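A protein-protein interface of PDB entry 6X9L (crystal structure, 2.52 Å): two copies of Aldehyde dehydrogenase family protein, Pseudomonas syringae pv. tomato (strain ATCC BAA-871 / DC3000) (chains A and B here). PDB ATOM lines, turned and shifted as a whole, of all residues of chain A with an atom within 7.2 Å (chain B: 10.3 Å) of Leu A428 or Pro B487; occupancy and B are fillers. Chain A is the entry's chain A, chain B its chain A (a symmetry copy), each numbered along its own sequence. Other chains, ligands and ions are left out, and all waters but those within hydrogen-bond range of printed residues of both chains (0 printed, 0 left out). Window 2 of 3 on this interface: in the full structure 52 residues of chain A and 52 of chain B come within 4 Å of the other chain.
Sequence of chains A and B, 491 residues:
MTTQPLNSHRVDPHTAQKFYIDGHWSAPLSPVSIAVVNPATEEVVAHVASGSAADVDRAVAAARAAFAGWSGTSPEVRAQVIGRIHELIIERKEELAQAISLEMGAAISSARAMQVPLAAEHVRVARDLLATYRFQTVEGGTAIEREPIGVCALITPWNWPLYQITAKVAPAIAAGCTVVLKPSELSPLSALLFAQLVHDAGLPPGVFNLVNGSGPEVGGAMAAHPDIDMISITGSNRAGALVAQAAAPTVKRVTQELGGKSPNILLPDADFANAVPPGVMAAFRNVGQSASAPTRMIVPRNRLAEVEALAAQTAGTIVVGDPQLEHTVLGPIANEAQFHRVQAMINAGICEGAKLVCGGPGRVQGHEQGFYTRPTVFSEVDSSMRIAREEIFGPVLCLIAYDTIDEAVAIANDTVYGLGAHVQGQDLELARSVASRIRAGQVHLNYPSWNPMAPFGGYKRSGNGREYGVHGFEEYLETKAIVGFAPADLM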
ATOM      1  N   ASP A 269     -32.871  15.929 -17.090  1.00  0.00           N
ATOM      2  CA  ASP A 269     -33.250  14.577 -17.554  1.00  0.00           C
ATOM      3  C   ASP A 269     -32.910  13.512 -16.523  1.00  0.00           C
ATOM      4  O   ASP A 269     -32.989  12.358 -16.860  1.00  0.00           O
ATOM      5  CB  ASP A 269     -32.582  14.276 -18.891  1.00  0.00           C
ATOM      6  CG  ASP A 269     -31.084  14.100 -18.801  1.00  0.00           C
ATOM      7  OD1 ASP A 269     -30.532  14.455 -17.785  1.00  0.00           O
ATOM      8  OD2 ASP A 269     -30.505  13.597 -19.742  1.00  0.00           O
ATOM      9  N   GLY A 425     -27.479  12.848 -14.421  1.00  0.00           N
ATOM     10  CA  GLY A 425     -28.060  13.043 -15.728  1.00  0.00           C
ATOM     11  C   GLY A 425     -28.299  11.724 -16.428  1.00  0.00           C
ATOM     12  O   GLY A 425     -27.541  10.768 -16.231  1.00  0.00           O
ATOM     13  N   GLN A 426     -29.359  11.661 -17.240  1.00  0.00           N
ATOM     14  CA  GLN A 426     -29.623  10.459 -18.017  1.00  0.00           C
ATOM     15  C   GLN A 426     -28.794  10.440 -19.300  1.00  0.00           C
ATOM     16  O   GLN A 426     -28.163   9.429 -19.620  1.00  0.00           O
ATOM     17  CB  GLN A 426     -31.121  10.341 -18.323  1.00  0.00           C
ATOM     18  CG  GLN A 426     -31.680   8.931 -18.105  1.00  0.00           C
ATOM     19  CD  GLN A 426     -32.812   8.879 -17.078  1.00  0.00           C
ATOM     20  OE1 GLN A 426     -33.643   9.787 -16.997  1.00  0.00           O
ATOM     21  NE2 GLN A 426     -32.843   7.809 -16.289  1.00  0.00           N
ATOM     22  N   ASP A 427     -28.779  11.541 -20.049  1.00  0.00           N
ATOM     23  CA  ASP A 427     -27.931  11.619 -21.235  1.00  0.00           C
ATOM     24  C   ASP A 427     -26.470  11.729 -20.805  1.00  0.00           C
ATOM     25  O   ASP A 427     -26.054  12.762 -20.270  1.00  0.00           O
ATOM     26  CB  ASP A 427     -28.330  12.803 -22.108  1.00  0.00           C
ATOM     27  CG  ASP A 427     -27.383  13.000 -23.278  1.00  0.00           C
ATOM     28  OD1 ASP A 427     -26.470  12.166 -23.440  1.00  0.00           O
ATOM     29  OD2 ASP A 427     -27.535  13.979 -24.039  1.00  0.00           O
ATOM     30  N   LEU A 428     -25.684  10.672 -21.072  1.00  0.00           N
ATOM     31  CA  LEU A 428     -24.291  10.619 -20.626  1.00  0.00           C
ATOM     32  C   LEU A 428     -23.421  11.621 -21.379  1.00  0.00           C
ATOM     33  O   LEU A 428     -22.507  12.214 -20.798  1.00  0.00           O
ATOM     34  CB  LEU A 428     -23.728   9.201 -20.788  1.00  0.00           C
ATOM     35  CG  LEU A 428     -22.272   8.897 -20.372  1.00  0.00           C
ATOM     36  CD1 LEU A 428     -22.101   8.927 -18.863  1.00  0.00           C
ATOM     37  CD2 LEU A 428     -21.801   7.556 -20.907  1.00  0.00           C
ATOM     38  N   GLU A 429     -23.672  11.809 -22.674  1.00  0.00           N
ATOM     39  CA  GLU A 429     -22.942  12.823 -23.427  1.00  0.00           C
ATOM     40  C   GLU A 429     -23.095  14.190 -22.771  1.00  0.00           C
ATOM     41  O   GLU A 429     -22.103  14.849 -22.442  1.00  0.00           O
ATOM     42  CB  GLU A 429     -23.421  12.839 -24.884  1.00  0.00           C
ATOM     43  CG  GLU A 429     -23.071  14.091 -25.648  1.00  0.00           C
ATOM     44  CD  GLU A 429     -23.461  14.018 -27.111  1.00  0.00           C
ATOM     45  OE1 GLU A 429     -24.674  13.956 -27.421  1.00  0.00           O
ATOM     46  OE2 GLU A 429     -22.549  14.025 -27.961  1.00  0.00           O
ATOM     47  N   LEU A 430     -24.336  14.614 -22.531  1.00  0.00           N
ATOM     48  CA  LEU A 430     -24.557  15.909 -21.902  1.00  0.00           C
ATOM     49  C   LEU A 430     -23.870  15.982 -20.545  1.00  0.00           C
ATOM     50  O   LEU A 430     -23.204  16.976 -20.233  1.00  0.00           O
ATOM     51  CB  LEU A 430     -26.053  16.181 -21.763  1.00  0.00           C
ATOM     52  CG  LEU A 430     -26.368  17.387 -20.872  1.00  0.00           C
ATOM     53  CD1 LEU A 430     -26.090  18.718 -21.568  1.00  0.00           C
ATOM     54  CD2 LEU A 430     -27.796  17.305 -20.398  1.00  0.00           C
ATOM     55  N   ALA A 431     -24.003  14.928 -19.735  1.00  0.00           N
ATOM     56  CA  ALA A 431     -23.418  14.935 -18.395  1.00  0.00           C
ATOM     57  C   ALA A 431     -21.892  15.076 -18.442  1.00  0.00           C
ATOM     58  O   ALA A 431     -21.301  15.773 -17.611  1.00  0.00           O
ATOM     59  CB  ALA A 431     -23.828  13.669 -17.647  1.00  0.00           C
ATOM     60  N   ARG A 432     -21.243  14.435 -19.416  1.00  0.00           N
ATOM     61  CA  ARG A 432     -19.801  14.605 -19.585  1.00  0.00           C
ATOM     62  C   ARG A 432     -19.446  16.050 -19.915  1.00  0.00           C
ATOM     63  O   ARG A 432     -18.544  16.636 -19.301  1.00  0.00           O
ATOM     64  CB  ARG A 432     -19.280  13.681 -20.683  1.00  0.00           C
ATOM     65  CG  ARG A 432     -19.172  12.257 -20.275  1.00  0.00           C
ATOM     66  CD  ARG A 432     -19.273  11.355 -21.481  1.00  0.00           C
ATOM     67  NE  ARG A 432     -18.651  10.062 -21.232  1.00  0.00           N
ATOM     68  CZ  ARG A 432     -18.963   8.944 -21.874  1.00  0.00           C
ATOM     69  NH1 ARG A 432     -19.912   8.950 -22.801  1.00  0.00           N
ATOM     70  NH2 ARG A 432     -18.325   7.818 -21.581  1.00  0.00           N
ATOM     71  N   SER A 433     -20.117  16.635 -20.911  1.00  0.00           N
ATOM     72  CA  SER A 433     -19.787  18.004 -21.287  1.00  0.00           C
ATOM     73  C   SER A 433     -19.960  18.964 -20.101  1.00  0.00           C
ATOM     74  O   SER A 433     -19.170  19.903 -19.943  1.00  0.00           O
ATOM     75  CB  SER A 433     -20.628  18.439 -22.492  1.00  0.00           C
ATOM     76  OG  SER A 433     -21.907  18.900 -22.095  1.00  0.00           O
ATOM     77  N   VAL A 434     -20.962  18.739 -19.248  1.00  0.00           N
ATOM     78  CA  VAL A 434     -21.103  19.574 -18.057  1.00  0.00           C
ATOM     79  C   VAL A 434     -19.930  19.345 -17.099  1.00  0.00           C
ATOM     80  O   VAL A 434     -19.356  20.304 -16.552  1.00  0.00           O
ATOM     81  CB  VAL A 434     -22.457  19.314 -17.364  1.00  0.00           C
ATOM     82  CG1 VAL A 434     -22.698  20.361 -16.273  1.00  0.00           C
ATOM     83  CG2 VAL A 434     -23.601  19.305 -18.375  1.00  0.00           C
ATOM     84  N   LEU A 445     -19.962  11.172 -11.996  1.00  0.00           N
ATOM     85  CA  LEU A 445     -21.162  11.052 -12.812  1.00  0.00           C
ATOM     86  C   LEU A 445     -22.047   9.926 -12.295  1.00  0.00           C
ATOM     87  O   LEU A 445     -21.607   8.770 -12.218  1.00  0.00           O
ATOM     88  CB  LEU A 445     -20.777  10.782 -14.257  1.00  0.00           C
ATOM     89  CG  LEU A 445     -19.754  11.749 -14.819  1.00  0.00           C
ATOM     90  CD1 LEU A 445     -19.498  11.390 -16.262  1.00  0.00           C
ATOM     91  CD2 LEU A 445     -20.275  13.175 -14.704  1.00  0.00           C
ATOM     92  N   ASN A 446     -23.296  10.259 -11.963  1.00  0.00           N
ATOM     93  CA  ASN A 446     -24.288   9.267 -11.547  1.00  0.00           C
ATOM     94  C   ASN A 446     -23.718   8.313 -10.490  1.00  0.00           C
ATOM     95  O   ASN A 446     -23.858   7.091 -10.572  1.00  0.00           O
ATOM     96  CB  ASN A 446     -24.810   8.496 -12.762  1.00  0.00           C
ATOM     97  CG  ASN A 446     -25.432   9.405 -13.804  1.00  0.00           C
ATOM     98  OD1 ASN A 446     -26.228  10.287 -13.485  1.00  0.00           O
ATOM     99  ND2 ASN A 446     -25.058   9.202 -15.061  1.00  0.00           N
ATOM    100  N   PRO A 448     -20.617   7.189  -9.312  1.00  0.00           N
ATOM    101  CA  PRO A 448     -19.655   6.100  -9.498  1.00  0.00           C
ATOM    102  C   PRO A 448     -19.068   5.673  -8.163  1.00  0.00           C
ATOM    103  O   PRO A 448     -19.167   6.372  -7.151  1.00  0.00           O
ATOM    104  CB  PRO A 448     -18.588   6.730 -10.394  1.00  0.00           C
ATOM    105  CG  PRO A 448     -18.600   8.166  -9.970  1.00  0.00           C
ATOM    106  CD  PRO A 448     -20.048   8.497  -9.666  1.00  0.00           C
ATOM    107  N   GLN B 136      -7.123  14.754 -22.997  1.00  0.00           N
ATOM    108  CA  GLN B 136      -7.967  13.777 -22.333  1.00  0.00           C
ATOM    109  C   GLN B 136      -7.383  12.380 -22.483  1.00  0.00           C
ATOM    110  O   GLN B 136      -6.806  12.039 -23.519  1.00  0.00           O
ATOM    111  CB  GLN B 136      -9.377  13.791 -22.897  1.00  0.00           C
ATOM    112  CG  GLN B 136     -10.275  12.749 -22.290  1.00  0.00           C
ATOM    113  CD  GLN B 136     -11.587  12.673 -23.003  1.00  0.00           C
ATOM    114  OE1 GLN B 136     -12.635  13.049 -22.462  1.00  0.00           O
ATOM    115  NE2 GLN B 136     -11.551  12.187 -24.240  1.00  0.00           N
ATOM    116  N   VAL B 138      -8.420   8.151 -21.120  1.00  0.00           N
ATOM    117  CA  VAL B 138      -9.505   7.338 -20.598  1.00  0.00           C
ATOM    118  C   VAL B 138      -8.900   6.038 -20.085  1.00  0.00           C
ATOM    119  O   VAL B 138      -8.339   5.258 -20.864  1.00  0.00           O
ATOM    120  CB  VAL B 138     -10.587   7.093 -21.657  1.00  0.00           C
ATOM    121  CG1 VAL B 138     -11.702   6.237 -21.109  1.00  0.00           C
ATOM    122  CG2 VAL B 138     -11.118   8.446 -22.153  1.00  0.00           C
ATOM    123  N   GLY B 140     -10.627   3.689 -18.229  1.00  0.00           N
ATOM    124  CA  GLY B 140     -11.664   2.746 -17.861  1.00  0.00           C
ATOM    125  C   GLY B 140     -13.021   3.417 -17.843  1.00  0.00           C
ATOM    126  O   GLY B 140     -13.540   3.783 -18.903  1.00  0.00           O
ATOM    127  N   GLY B 141     -13.611   3.570 -16.653  1.00  0.00           N
ATOM    128  CA  GLY B 141     -14.726   4.462 -16.418  1.00  0.00           C
ATOM    129  C   GLY B 141     -14.317   5.836 -15.937  1.00  0.00           C
ATOM    130  O   GLY B 141     -15.184   6.666 -15.653  1.00  0.00           O
ATOM    131  N   THR B 142     -13.011   6.104 -15.826  1.00  0.00           N
ATOM    132  CA  THR B 142     -12.492   7.391 -15.376  1.00  0.00           C
ATOM    133  C   THR B 142     -11.702   8.035 -16.500  1.00  0.00           C
ATOM    134  O   THR B 142     -10.907   7.369 -17.165  1.00  0.00           O
ATOM    135  CB  THR B 142     -11.583   7.250 -14.128  1.00  0.00           C
ATOM    136  OG1 THR B 142     -12.366   6.858 -12.990  1.00  0.00           O
ATOM    137  CG2 THR B 142     -10.868   8.571 -13.821  1.00  0.00           C
ATOM    138  N   ALA B 143     -11.919   9.329 -16.710  1.00  0.00           N
ATOM    139  CA  ALA B 143     -11.211  10.093 -17.727  1.00  0.00           C
ATOM    140  C   ALA B 143     -10.431  11.221 -17.061  1.00  0.00           C
ATOM    141  O   ALA B 143     -10.934  11.880 -16.145  1.00  0.00           O
ATOM    142  CB  ALA B 143     -12.176  10.674 -18.779  1.00  0.00           C
ATOM    143  N   GLU B 145      -8.766  14.797 -17.734  1.00  0.00           N
ATOM    144  CA  GLU B 145      -8.734  15.939 -18.632  1.00  0.00           C
ATOM    145  C   GLU B 145      -7.760  16.972 -18.082  1.00  0.00           C
ATOM    146  O   GLU B 145      -7.794  17.288 -16.896  1.00  0.00           O
ATOM    147  CB  GLU B 145     -10.134  16.521 -18.815  1.00  0.00           C
ATOM    148  CG  GLU B 145     -11.101  15.515 -19.456  1.00  0.00           C
ATOM    149  CD  GLU B 145     -12.429  16.135 -19.866  1.00  0.00           C
ATOM    150  OE1 GLU B 145     -12.561  17.374 -19.756  1.00  0.00           O
ATOM    151  OE2 GLU B 145     -13.331  15.384 -20.298  1.00  0.00           O
ATOM    152  N   ILE B 482     -12.668  12.598 -14.102  1.00  0.00           N
ATOM    153  CA  ILE B 482     -14.099  12.408 -14.270  1.00  0.00           C
ATOM    154  C   ILE B 482     -14.376  10.937 -14.030  1.00  0.00           C
ATOM    155  O   ILE B 482     -14.308  10.131 -14.966  1.00  0.00           O
ATOM    156  CB  ILE B 482     -14.568  12.867 -15.658  1.00  0.00           C
ATOM    157  CG1 ILE B 482     -14.155  14.313 -15.872  1.00  0.00           C
ATOM    158  CG2 ILE B 482     -16.089  12.735 -15.792  1.00  0.00           C
ATOM    159  CD1 ILE B 482     -14.516  14.823 -17.226  1.00  0.00           C
ATOM    160  N   VAL B 483     -14.662  10.581 -12.765  1.00  0.00           N
ATOM    161  CA  VAL B 483     -14.987   9.209 -12.389  1.00  0.00           C
ATOM    162  C   VAL B 483     -16.428   8.911 -12.793  1.00  0.00           C
ATOM    163  O   VAL B 483     -17.305   9.780 -12.708  1.00  0.00           O
ATOM    164  CB  VAL B 483     -14.773   8.986 -10.876  1.00  0.00           C
ATOM    165  CG1 VAL B 483     -14.624   7.501 -10.584  1.00  0.00           C
ATOM    166  CG2 VAL B 483     -13.552   9.763 -10.358  1.00  0.00           C
ATOM    167  N   GLY B 484     -16.684   7.681 -13.238  1.00  0.00           N
ATOM    168  CA  GLY B 484     -17.967   7.383 -13.842  1.00  0.00           C
ATOM    169  C   GLY B 484     -18.128   7.921 -15.249  1.00  0.00           C
ATOM    170  O   GLY B 484     -19.256   8.050 -15.731  1.00  0.00           O
ATOM    171  N   PHE B 485     -17.021   8.268 -15.908  1.00  0.00           N
ATOM    172  CA  PHE B 485     -17.056   8.721 -17.298  1.00  0.00           C
ATOM    173  C   PHE B 485     -17.705   7.678 -18.196  1.00  0.00           C
ATOM    174  O   PHE B 485     -18.514   8.017 -19.064  1.00  0.00           O
ATOM    175  CB  PHE B 485     -15.625   9.028 -17.747  1.00  0.00           C
ATOM    176  CG  PHE B 485     -15.509   9.632 -19.108  1.00  0.00           C
ATOM    177  CD1 PHE B 485     -15.742  10.978 -19.305  1.00  0.00           C
ATOM    178  CD2 PHE B 485     -15.088   8.865 -20.186  1.00  0.00           C
ATOM    179  CE1 PHE B 485     -15.597  11.544 -20.558  1.00  0.00           C
ATOM    180  CE2 PHE B 485     -14.942   9.422 -21.436  1.00  0.00           C
ATOM    181  CZ  PHE B 485     -15.199  10.765 -21.626  1.00  0.00           C
ATOM    182  N   ALA B 486     -17.358   6.403 -18.006  1.00  0.00           N
ATOM    183  CA  ALA B 486     -18.088   5.283 -18.596  1.00  0.00           C
ATOM    184  C   ALA B 486     -18.737   4.464 -17.488  1.00  0.00           C
ATOM    185  O   ALA B 486     -18.027   3.974 -16.598  1.00  0.00           O
ATOM    186  CB  ALA B 486     -17.157   4.407 -19.429  1.00  0.00           C
ATOM    187  N   PRO B 487     -20.060   4.301 -17.484  1.00  0.00           N
ATOM    188  CA  PRO B 487     -20.709   3.491 -16.439  1.00  0.00           C
ATOM    189  C   PRO B 487     -20.080   2.108 -16.316  1.00  0.00           C
ATOM    190  O   PRO B 487     -19.549   1.560 -17.282  1.00  0.00           O
ATOM    191  CB  PRO B 487     -22.166   3.397 -16.911  1.00  0.00           C
ATOM    192  CG  PRO B 487     -22.361   4.605 -17.778  1.00  0.00           C
ATOM    193  CD  PRO B 487     -21.028   4.908 -18.414  1.00  0.00           C
ATOM    194  N   ALA B 488     -20.161   1.542 -15.113  1.00  0.00           N
ATOM    195  CA  ALA B 488     -19.510   0.280 -14.784  1.00  0.00           C
ATOM    196  C   ALA B 488     -20.436  -0.906 -15.064  1.00  0.00           C
ATOM    197  O   ALA B 488     -21.603  -0.745 -15.427  1.00  0.00           O
ATOM    198  CB  ALA B 488     -19.054   0.283 -13.322  1.00  0.00           C
ATOM    199  N   ASP B 489     -19.897  -2.114 -14.889  1.00  0.00           N
ATOM    200  CA  ASP B 489     -20.619  -3.330 -15.253  1.00  0.00           C
ATOM    201  C   ASP B 489     -21.712  -3.670 -14.233  1.00  0.00           C
ATOM    202  O   ASP B 489     -21.739  -3.162 -13.106  1.00  0.00           O
ATOM    203  CB  ASP B 489     -19.653  -4.515 -15.378  1.00  0.00           C
ATOM    204  CG  ASP B 489     -18.767  -4.443 -16.621  1.00  0.00           C
ATOM    205  OD1 ASP B 489     -19.236  -3.952 -17.669  1.00  0.00           O
ATOM    206  OD2 ASP B 489     -17.599  -4.896 -16.550  1.00  0.00           O
ATOM    207  N   LEU B 490     -22.611  -4.566 -14.645  1.00  0.00           N
ATOM    208  CA  LEU B 490     -23.712  -5.083 -13.821  1.00  0.00           C
ATOM    209  C   LEU B 490     -24.957  -4.225 -14.025  1.00  0.00           C
ATOM    210  O   LEU B 490     -25.275  -3.845 -15.153  1.00  0.00           O
ATOM    211  CB  LEU B 490     -23.333  -5.141 -12.332  1.00  0.00           C
ATOM    212  CG  LEU B 490     -23.221  -6.513 -11.665  1.00  0.00           C
ATOM    213  CD1 LEU B 490     -21.837  -6.705 -11.061  1.00  0.00           C
ATOM    214  CD2 LEU B 490     -24.289  -6.671 -10.604  1.00  0.00           C
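Printed residues of chain A that touch a printed residue of chain B: Leu A428, Arg A432, Leu A445 and Pro A448. Hydrophobic or aromatic side chains of chain B within 4 Å of the printed part of chain A: Ile B482, Phe B485 and Pro B487. Among the printed residues, 10 pairs touch across the chains. Among the printed residues, no Asp or Glu carboxylate lies within 4 Å of a Lys or Arg side-chain nitrogen of the other chain.
The backbone carbonyl oxygen (O) of Val B483 lies within hydrogen-bond range of the backbone NH (N) of Leu A445 (3.1 Å). The guanidinium group (NH2) of Arg A432 sits at hydrogen-bond distance from the backbone carbonyl oxygen (O) of Phe B485, at 2.5 Å.
Of chain B, only Phe B485 and Pro B487 come within 4 Å of Leu A428. No residue of chain B comes within 4 Å of Ala A431. Of chain B, only Phe B485 (2.5 Å) and Ala B486 (3.9 Å) come within 4 Å of Arg A432. Ala B143 touches none of the printed residues of chain A. Glu B145 touches none of the printed residues of chain A. Of the printed residues of chain A, Ile B482 touches Leu A445. Of the printed residues of chain A, Val B483 touches Leu A445 and Pro A448. Of the printed residues of chain A, Gly B484 touches Leu A445 and Pro A448. Of the printed residues of chain A, Phe B485 touches Leu A428, Arg A432 and Leu A445. Printed residues of chain A within 4 Å of Ala B486: Arg A432 (3.9 Å). Pro B487 touches just one residue of chain A: Leu A428 (3.7 Å). The nearest printed residue of chain A that does not touch Gly B484 is Leu A428 (4.3 Å).
Among the printed residues, pairs that only touch across the chains: Leu A428 with Phe B485 (3.7 Å), Leu A428 with Pro B487 (3.7 Å), Arg A432 with Ala B486 (3.9 Å), Leu A445 with Ile B482 (3.7 Å), Leu A445 with Gly B484 (3.4 Å), Leu A445 with Phe B485 (3.8 Å), Pro A448 with Val B483 (3.4 Å) and Pro A448 with Gly B484 (3.6 Å).
O of Gly B141 lies within hydrogen-bond range of N of Gly B484. The backbone carbonyl oxygen of Gly B141 lies within hydrogen-bond range of the backbone NH of Phe B485 (2.5 Å). The backbone NH of Ile B482 sits at hydrogen-bond distance from the backbone carbonyl oxygen of Ala B143 (2.8 Å). O of Gly B141 is in hydrogen-bond range of N of Ala B486, 3.2 Å away.
No position is printed for both chains. Of the 10 pairs that touch across the chains among the printed residues, none has its exchanged pair printed and touching as well.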
